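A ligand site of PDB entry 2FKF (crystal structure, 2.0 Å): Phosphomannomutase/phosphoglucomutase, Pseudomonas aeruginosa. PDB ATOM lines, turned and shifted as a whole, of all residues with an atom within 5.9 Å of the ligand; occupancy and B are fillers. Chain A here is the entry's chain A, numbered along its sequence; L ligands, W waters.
Hydrophobic or aromatic side chains within 4 Å of the ligand: His 108. The nearest printed residue that does not touch the ligand is Lys 284 (4.2 Å).
The guanidinium group (NH2) of Arg 19 is in salt-bridge range of the side-chain carboxylate (OD2) of Asp 17 (2.9 Å). NH2 of Arg 420 lies within hydrogen-bond range of OG1 of Thr 305 (3.3 Å). N of Ser 326 lies close to OE1 of Glu 324 (3.3 Å). The side-chain hydroxyl (OH) of Tyr 16 lies within hydrogen-bond range of the side-chain amide nitrogen (ND2) of Asn 423 (3.4 Å). The side-chain hydroxyl (OG) of Ser 422 sits at hydrogen-bond distance from the side-chain hydroxyl (OG1) of Thr 425. The side-chain amide oxygen (OD1) of Asn 109 is in hydrogen-bond range of the guanidinium group (NH1) of Arg 19 (2.7 Å). O2P of SEP 107 lies within salt-bridge range of the guanidinium group (NH2) of Arg 19 (2.9 Å). The backbone carbonyl oxygen (O) of Arg 420 is in hydrogen-bond range of the backbone NH (N) of Val 429, 2.8 Å away.
Water W3 lies within hydrogen-bond range of O3 of the ligand and OE1 of Glu 324. Water W9 lies within hydrogen-bond range of the side-chain amide oxygen of Asn 109 and an oxygen (O8) of the ligand. Water W6 lies within hydrogen-bond range of OG1 of Thr 305 (2.7 Å), O12 of the ligand (3.0 Å) and NH2 of Arg 420 (3.4 Å). Water W8 lies within hydrogen-bond range of the side-chain amino group of Lys 284 (2.6 Å), the side-chain hydroxyl of Ser 326 (2.7 Å) and an oxygen (O2) of the ligand (3.4 Å).
An oxygen (O8) of the ligand lies within salt-bridge range of the guanidinium group of Arg 14, at 2.9 Å. An oxygen (O3) of the ligand is in hydrogen-bond range of the side-chain hydroxyl (OG) of Ser 326 (2.8 Å). OG1 of Thr 424 lies within hydrogen-bond range of O11 of the ligand (2.7 Å). A ring nitrogen (NE2) of His 108 sits at hydrogen-bond distance from an oxygen (O9) of the ligand. OG of Ser 422 sits at hydrogen-bond distance from O10 of the ligand (2.6 Å). The guanidinium group of Arg 19 lies within salt-bridge range of an oxygen (O7) of the ligand (3.0 Å). An oxygen (O12) of the ligand lies within salt-bridge range of the guanidinium group (NH1) of Arg 420 (3.0 Å). N of Asn 423 sits at hydrogen-bond distance from O12 of the ligand, 3.0 Å away. N of Thr 424 sits at hydrogen-bond distance from O11 of the ligand (3.2 Å). ND2 of Asn 109 is in hydrogen-bond range of O9 of the ligand (3.0 Å).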
ATOM      1  N   ARG A  14       0.145  13.889 -21.336  1.00  0.00           N
ATOM      2  CA  ARG A  14      -0.217  15.302 -21.218  1.00  0.00           C
ATOM      3  C   ARG A  14       0.913  16.231 -21.648  1.00  0.00           C
ATOM      4  O   ARG A  14       1.941  15.783 -22.147  1.00  0.00           O
ATOM      5  CB  ARG A  14      -0.633  15.601 -19.778  1.00  0.00           C
ATOM      6  CG  ARG A  14      -1.647  14.596 -19.221  1.00  0.00           C
ATOM      7  CD  ARG A  14      -2.500  15.193 -18.124  1.00  0.00           C
ATOM      8  NE  ARG A  14      -1.690  15.577 -16.976  1.00  0.00           N
ATOM      9  CZ  ARG A  14      -2.156  16.227 -15.910  1.00  0.00           C
ATOM     10  NH1 ARG A  14      -3.430  16.548 -15.822  1.00  0.00           N
ATOM     11  NH2 ARG A  14      -1.335  16.537 -14.916  1.00  0.00           N
ATOM     12  N   TYR A  16       2.957  18.300 -19.848  1.00  0.00           N
ATOM     13  CA  TYR A  16       4.175  18.347 -19.008  1.00  0.00           C
ATOM     14  C   TYR A  16       4.406  17.068 -18.186  1.00  0.00           C
ATOM     15  O   TYR A  16       5.335  17.008 -17.378  1.00  0.00           O
ATOM     16  CB  TYR A  16       4.113  19.590 -18.106  1.00  0.00           C
ATOM     17  CG  TYR A  16       3.591  20.808 -18.844  1.00  0.00           C
ATOM     18  CD1 TYR A  16       4.124  21.169 -20.084  1.00  0.00           C
ATOM     19  CD2 TYR A  16       2.538  21.584 -18.330  1.00  0.00           C
ATOM     20  CE1 TYR A  16       3.642  22.268 -20.784  1.00  0.00           C
ATOM     21  CE2 TYR A  16       2.051  22.695 -19.024  1.00  0.00           C
ATOM     22  CZ  TYR A  16       2.602  23.025 -20.253  1.00  0.00           C
ATOM     23  OH  TYR A  16       2.134  24.108 -20.959  1.00  0.00           O
ATOM     24  N   ASP A  17       3.581  16.051 -18.398  1.00  0.00           N
ATOM     25  CA  ASP A  17       3.732  14.786 -17.682  1.00  0.00           C
ATOM     26  C   ASP A  17       2.823  13.700 -18.236  1.00  0.00           C
ATOM     27  O   ASP A  17       2.151  13.882 -19.250  1.00  0.00           O
ATOM     28  CB  ASP A  17       3.439  14.977 -16.182  1.00  0.00           C
ATOM     29  CG  ASP A  17       2.037  15.452 -15.917  1.00  0.00           C
ATOM     30  OD1 ASP A  17       1.184  15.389 -16.840  1.00  0.00           O
ATOM     31  OD2 ASP A  17       1.761  15.882 -14.778  1.00  0.00           O
ATOM     32  N   ARG A  19      -0.283  11.311 -16.623  1.00  0.00           N
ATOM     33  CA  ARG A  19      -1.194  11.285 -15.484  1.00  0.00           C
ATOM     34  C   ARG A  19      -2.452  10.512 -15.874  1.00  0.00           C
ATOM     35  O   ARG A  19      -3.028  10.772 -16.941  1.00  0.00           O
ATOM     36  CB  ARG A  19      -1.590  12.710 -15.086  1.00  0.00           C
ATOM     37  CG  ARG A  19      -2.357  12.821 -13.762  1.00  0.00           C
ATOM     38  CD  ARG A  19      -1.448  12.627 -12.552  1.00  0.00           C
ATOM     39  NE  ARG A  19      -0.351  13.598 -12.535  1.00  0.00           N
ATOM     40  CZ  ARG A  19      -0.441  14.855 -12.078  1.00  0.00           C
ATOM     41  NH1 ARG A  19      -1.584  15.318 -11.597  1.00  0.00           N
ATOM     42  NH2 ARG A  19       0.610  15.643 -12.131  1.00  0.00           N
ATOM     43  N   SEP A 107       0.908  13.656  -7.966  1.00  0.00           N
ATOM     44  CA  SEP A 107       0.982  15.019  -7.434  1.00  0.00           C
ATOM     45  CB  SEP A 107       0.805  16.016  -8.588  1.00  0.00           C
ATOM     46  OG  SEP A 107       0.766  17.352  -8.125  1.00  0.00           O
ATOM     47  C   SEP A 107       0.003  15.259  -6.261  1.00  0.00           C
ATOM     48  O   SEP A 107       0.173  14.688  -5.173  1.00  0.00           O
ATOM     49  P   SEP A 107       1.470  18.435  -9.120  1.00  0.00           P
ATOM     50  O1P SEP A 107       0.503  19.707  -9.260  1.00  0.00           O
ATOM     51  O2P SEP A 107       1.788  17.809 -10.554  1.00  0.00           O
ATOM     52  O3P SEP A 107       2.816  18.907  -8.410  1.00  0.00           O
ATOM     53  N   HIS A 108      -1.026  16.072  -6.492  1.00  0.00           N
ATOM     54  CA  HIS A 108      -2.003  16.400  -5.448  1.00  0.00           C
ATOM     55  C   HIS A 108      -3.379  15.798  -5.720  1.00  0.00           C
ATOM     56  O   HIS A 108      -4.332  16.071  -4.998  1.00  0.00           O
ATOM     57  CB  HIS A 108      -2.119  17.925  -5.310  1.00  0.00           C
ATOM     58  CG  HIS A 108      -2.688  18.588  -6.526  1.00  0.00           C
ATOM     59  ND1 HIS A 108      -4.037  18.661  -6.768  1.00  0.00           N
ATOM     60  CD2 HIS A 108      -2.077  19.176  -7.583  1.00  0.00           C
ATOM     61  CE1 HIS A 108      -4.244  19.288  -7.920  1.00  0.00           C
ATOM     62  NE2 HIS A 108      -3.070  19.616  -8.432  1.00  0.00           N
ATOM     63  N   ASN A 109      -3.491  14.982  -6.756  1.00  0.00           N
ATOM     64  CA  ASN A 109      -4.778  14.396  -7.173  1.00  0.00           C
ATOM     65  C   ASN A 109      -5.321  13.389  -6.148  1.00  0.00           C
ATOM     66  O   ASN A 109      -4.602  13.007  -5.220  1.00  0.00           O
ATOM     67  CB  ASN A 109      -4.621  13.743  -8.543  1.00  0.00           C
ATOM     68  CG  ASN A 109      -4.394  14.765  -9.666  1.00  0.00           C
ATOM     69  OD1 ASN A 109      -3.978  14.390 -10.772  1.00  0.00           O
ATOM     70  ND2 ASN A 109      -4.678  16.030  -9.393  1.00  0.00           N
ATOM     71  N   LYS A 284       0.589  34.895 -14.691  1.00  0.00           N
ATOM     72  CA  LYS A 284      -0.423  35.111 -13.656  1.00  0.00           C
ATOM     73  C   LYS A 284       0.121  35.901 -12.440  1.00  0.00           C
ATOM     74  O   LYS A 284      -0.618  36.140 -11.481  1.00  0.00           O
ATOM     75  CB  LYS A 284      -0.961  33.759 -13.180  1.00  0.00           C
ATOM     76  CG  LYS A 284      -1.604  32.953 -14.280  1.00  0.00           C
ATOM     77  CD  LYS A 284      -1.881  31.518 -13.843  1.00  0.00           C
ATOM     78  CE  LYS A 284      -3.267  31.374 -13.261  1.00  0.00           C
ATOM     79  NZ  LYS A 284      -3.513  29.977 -12.839  1.00  0.00           N
ATOM     80  N   THR A 305       2.831  29.690 -18.146  1.00  0.00           N
ATOM     81  CA  THR A 305       2.490  28.798 -17.029  1.00  0.00           C
ATOM     82  C   THR A 305       2.980  27.385 -17.313  1.00  0.00           C
ATOM     83  O   THR A 305       3.151  27.012 -18.476  1.00  0.00           O
ATOM     84  CB  THR A 305       0.956  28.745 -16.761  1.00  0.00           C
ATOM     85  OG1 THR A 305       0.249  28.342 -17.948  1.00  0.00           O
ATOM     86  CG2 THR A 305       0.439  30.110 -16.332  1.00  0.00           C
ATOM     87  N   GLU A 324       6.131  30.197 -10.130  1.00  0.00           N
ATOM     88  CA  GLU A 324       4.847  30.427 -10.744  1.00  0.00           C
ATOM     89  C   GLU A 324       3.714  30.335  -9.747  1.00  0.00           C
ATOM     90  O   GLU A 324       3.877  29.838  -8.627  1.00  0.00           O
ATOM     91  CB  GLU A 324       4.647  29.477 -11.919  1.00  0.00           C
ATOM     92  CG  GLU A 324       4.930  28.056 -11.638  1.00  0.00           C
ATOM     93  CD  GLU A 324       3.719  27.346 -11.122  1.00  0.00           C
ATOM     94  OE1 GLU A 324       2.679  27.346 -11.822  1.00  0.00           O
ATOM     95  OE2 GLU A 324       3.788  26.775 -10.006  1.00  0.00           O
ATOM     96  N   SER A 326       1.124  28.566  -9.190  1.00  0.00           N
ATOM     97  CA  SER A 326       0.693  27.298  -8.576  1.00  0.00           C
ATOM     98  C   SER A 326       1.595  26.846  -7.433  1.00  0.00           C
ATOM     99  O   SER A 326       1.312  25.826  -6.809  1.00  0.00           O
ATOM    100  CB  SER A 326       0.540  26.201  -9.631  1.00  0.00           C
ATOM    101  OG  SER A 326      -0.534  26.503 -10.497  1.00  0.00           O
ATOM    102  N   HIS A 328       5.118  26.361  -7.461  1.00  0.00           N
ATOM    103  CA  HIS A 328       6.413  25.806  -7.801  1.00  0.00           C
ATOM    104  C   HIS A 328       7.474  26.926  -7.776  1.00  0.00           C
ATOM    105  O   HIS A 328       7.336  27.931  -8.468  1.00  0.00           O
ATOM    106  CB  HIS A 328       6.376  25.146  -9.181  1.00  0.00           C
ATOM    107  CG  HIS A 328       5.580  23.881  -9.256  1.00  0.00           C
ATOM    108  ND1 HIS A 328       4.259  23.850  -9.641  1.00  0.00           N
ATOM    109  CD2 HIS A 328       5.946  22.599  -9.044  1.00  0.00           C
ATOM    110  CE1 HIS A 328       3.833  22.588  -9.637  1.00  0.00           C
ATOM    111  NE2 HIS A 328       4.846  21.815  -9.275  1.00  0.00           N
ATOM    112  N   ARG A 420      -6.629  33.168 -20.395  1.00  0.00           N
ATOM    113  CA  ARG A 420      -5.954  32.062 -21.038  1.00  0.00           C
ATOM    114  C   ARG A 420      -6.841  30.824 -21.004  1.00  0.00           C
ATOM    115  O   ARG A 420      -7.778  30.731 -20.212  1.00  0.00           O
ATOM    116  CB  ARG A 420      -4.614  31.792 -20.357  1.00  0.00           C
ATOM    117  CG  ARG A 420      -4.735  31.345 -18.919  1.00  0.00           C
ATOM    118  CD  ARG A 420      -3.416  30.851 -18.375  1.00  0.00           C
ATOM    119  NE  ARG A 420      -2.900  29.672 -19.068  1.00  0.00           N
ATOM    120  CZ  ARG A 420      -3.091  28.402 -18.719  1.00  0.00           C
ATOM    121  NH1 ARG A 420      -3.827  28.079 -17.659  1.00  0.00           N
ATOM    122  NH2 ARG A 420      -2.533  27.439 -19.434  1.00  0.00           N
ATOM    123  N   ALA A 421      -6.532  29.871 -21.871  1.00  0.00           N
ATOM    124  CA  ALA A 421      -7.270  28.611 -21.936  1.00  0.00           C
ATOM    125  C   ALA A 421      -6.543  27.648 -21.041  1.00  0.00           C
ATOM    126  O   ALA A 421      -5.328  27.567 -21.084  1.00  0.00           O
ATOM    127  CB  ALA A 421      -7.303  28.067 -23.377  1.00  0.00           C
ATOM    128  N   SER A 422      -7.291  26.936 -20.208  1.00  0.00           N
ATOM    129  CA  SER A 422      -6.736  25.873 -19.410  1.00  0.00           C
ATOM    130  C   SER A 422      -6.273  24.781 -20.350  1.00  0.00           C
ATOM    131  O   SER A 422      -7.010  24.419 -21.263  1.00  0.00           O
ATOM    132  CB  SER A 422      -7.795  25.329 -18.441  1.00  0.00           C
ATOM    133  OG  SER A 422      -7.461  24.037 -17.975  1.00  0.00           O
ATOM    134  N   ASN A 423      -5.078  24.249 -20.144  1.00  0.00           N
ATOM    135  CA  ASN A 423      -4.625  23.119 -20.963  1.00  0.00           C
ATOM    136  C   ASN A 423      -5.468  21.863 -20.729  1.00  0.00           C
ATOM    137  O   ASN A 423      -5.792  21.163 -21.677  1.00  0.00           O
ATOM    138  CB  ASN A 423      -3.146  22.815 -20.736  1.00  0.00           C
ATOM    139  CG  ASN A 423      -2.249  23.924 -21.231  1.00  0.00           C
ATOM    140  OD1 ASN A 423      -2.446  24.486 -22.309  1.00  0.00           O
ATOM    141  ND2 ASN A 423      -1.244  24.257 -20.430  1.00  0.00           N
ATOM    142  N   THR A 424      -5.832  21.595 -19.470  1.00  0.00           N
ATOM    143  CA  THR A 424      -6.401  20.288 -19.100  1.00  0.00           C
ATOM    144  C   THR A 424      -7.921  20.259 -18.973  1.00  0.00           C
ATOM    145  O   THR A 424      -8.503  19.175 -19.009  1.00  0.00           O
ATOM    146  CB  THR A 424      -5.796  19.789 -17.768  1.00  0.00           C
ATOM    147  OG1 THR A 424      -5.941  20.783 -16.745  1.00  0.00           O
ATOM    148  CG2 THR A 424      -4.314  19.495 -17.966  1.00  0.00           C
ATOM    149  N   THR A 425      -8.556  21.422 -18.835  1.00  0.00           N
ATOM    150  CA  THR A 425     -10.011  21.483 -18.604  1.00  0.00           C
ATOM    151  C   THR A 425     -10.644  22.426 -19.615  1.00  0.00           C
ATOM    152  O   THR A 425      -9.958  23.270 -20.164  1.00  0.00           O
ATOM    153  CB  THR A 425     -10.305  21.956 -17.148  1.00  0.00           C
ATOM    154  OG1 THR A 425      -9.800  23.270 -16.956  1.00  0.00           O
ATOM    155  CG2 THR A 425      -9.634  21.042 -16.142  1.00  0.00           C
ATOM    156  N   VAL A 429      -9.424  30.895 -17.936  1.00  0.00           N
ATOM    157  CA  VAL A 429      -8.922  31.317 -16.647  1.00  0.00           C
ATOM    158  C   VAL A 429      -8.544  32.790 -16.730  1.00  0.00           C
ATOM    159  O   VAL A 429      -7.815  33.174 -17.655  1.00  0.00           O
ATOM    160  CB  VAL A 429      -7.653  30.541 -16.249  1.00  0.00           C
ATOM    161  CG1 VAL A 429      -7.130  31.033 -14.871  1.00  0.00           C
ATOM    162  CG2 VAL A 429      -7.910  29.041 -16.240  1.00  0.00           C
HETATM  163  C1  LIG L   1      -3.775  24.058 -14.041  1.00  0.00           C
HETATM  164  C2  LIG L   1      -2.794  24.490 -12.939  1.00  0.00           C
HETATM  165  C3  LIG L   1      -1.459  23.798 -13.131  1.00  0.00           C
HETATM  166  C4  LIG L   1      -1.701  22.304 -13.088  1.00  0.00           C
HETATM  167  C5  LIG L   1      -2.739  21.895 -14.133  1.00  0.00           C
HETATM  168  C6  LIG L   1      -3.068  20.407 -14.079  1.00  0.00           C
HETATM  169  O1  LIG L   1      -3.299  24.413 -15.341  1.00  0.00           O
HETATM  170  O2  LIG L   1      -2.610  25.893 -12.936  1.00  0.00           O
HETATM  171  O3  LIG L   1      -0.529  24.189 -12.134  1.00  0.00           O
HETATM  172  O4  LIG L   1      -0.464  21.660 -13.332  1.00  0.00           O
HETATM  173  O5  LIG L   1      -3.935  22.640 -13.971  1.00  0.00           O
HETATM  174  O6  LIG L   1      -3.697  20.101 -12.849  1.00  0.00           O
HETATM  175  P1  LIG L   1      -3.777  18.631 -12.489  1.00  0.00           P
HETATM  176  O7  LIG L   1      -2.395  18.067 -12.374  1.00  0.00           O
HETATM  177  O8  LIG L   1      -4.566  17.874 -13.510  1.00  0.00           O
HETATM  178  O9  LIG L   1      -4.444  18.454 -11.141  1.00  0.00           O
HETATM  179  P2  LIG L   1      -4.121  24.179 -16.584  1.00  0.00           P
HETATM  180  O10 LIG L   1      -5.554  24.548 -16.322  1.00  0.00           O
HETATM  181  O11 LIG L   1      -4.086  22.748 -17.046  1.00  0.00           O
HETATM  182  O12 LIG L   1      -3.558  25.069 -17.663  1.00  0.00           O
HETATM  183  O   HOH W   1      -7.038  23.515 -14.329  1.00  0.00           O
HETATM  184  O   HOH W   2      -5.475  21.068 -10.552  1.00  0.00           O
HETATM  185  O   HOH W   3       1.789  24.876 -13.075  1.00  0.00           O
HETATM  186  O   HOH W   4      -1.582  22.019 -17.737  1.00  0.00           O
HETATM  187  O   HOH W   5      -1.639  27.290 -14.812  1.00  0.00           O
HETATM  188  O   HOH W   6      -0.773  26.015 -16.901  1.00  0.00           O
HETATM  189  O   HOH W   7      -5.688  26.754 -14.884  1.00  0.00           O
HETATM  190  O   HOH W   8      -1.651  28.729 -11.428  1.00  0.00           O
HETATM  191  O   HOH W   9      -5.374  15.221 -12.940  1.00  0.00           O
HETATM  192  O   HOH W  10      -6.139  21.567 -12.841  1.00  0.00           O
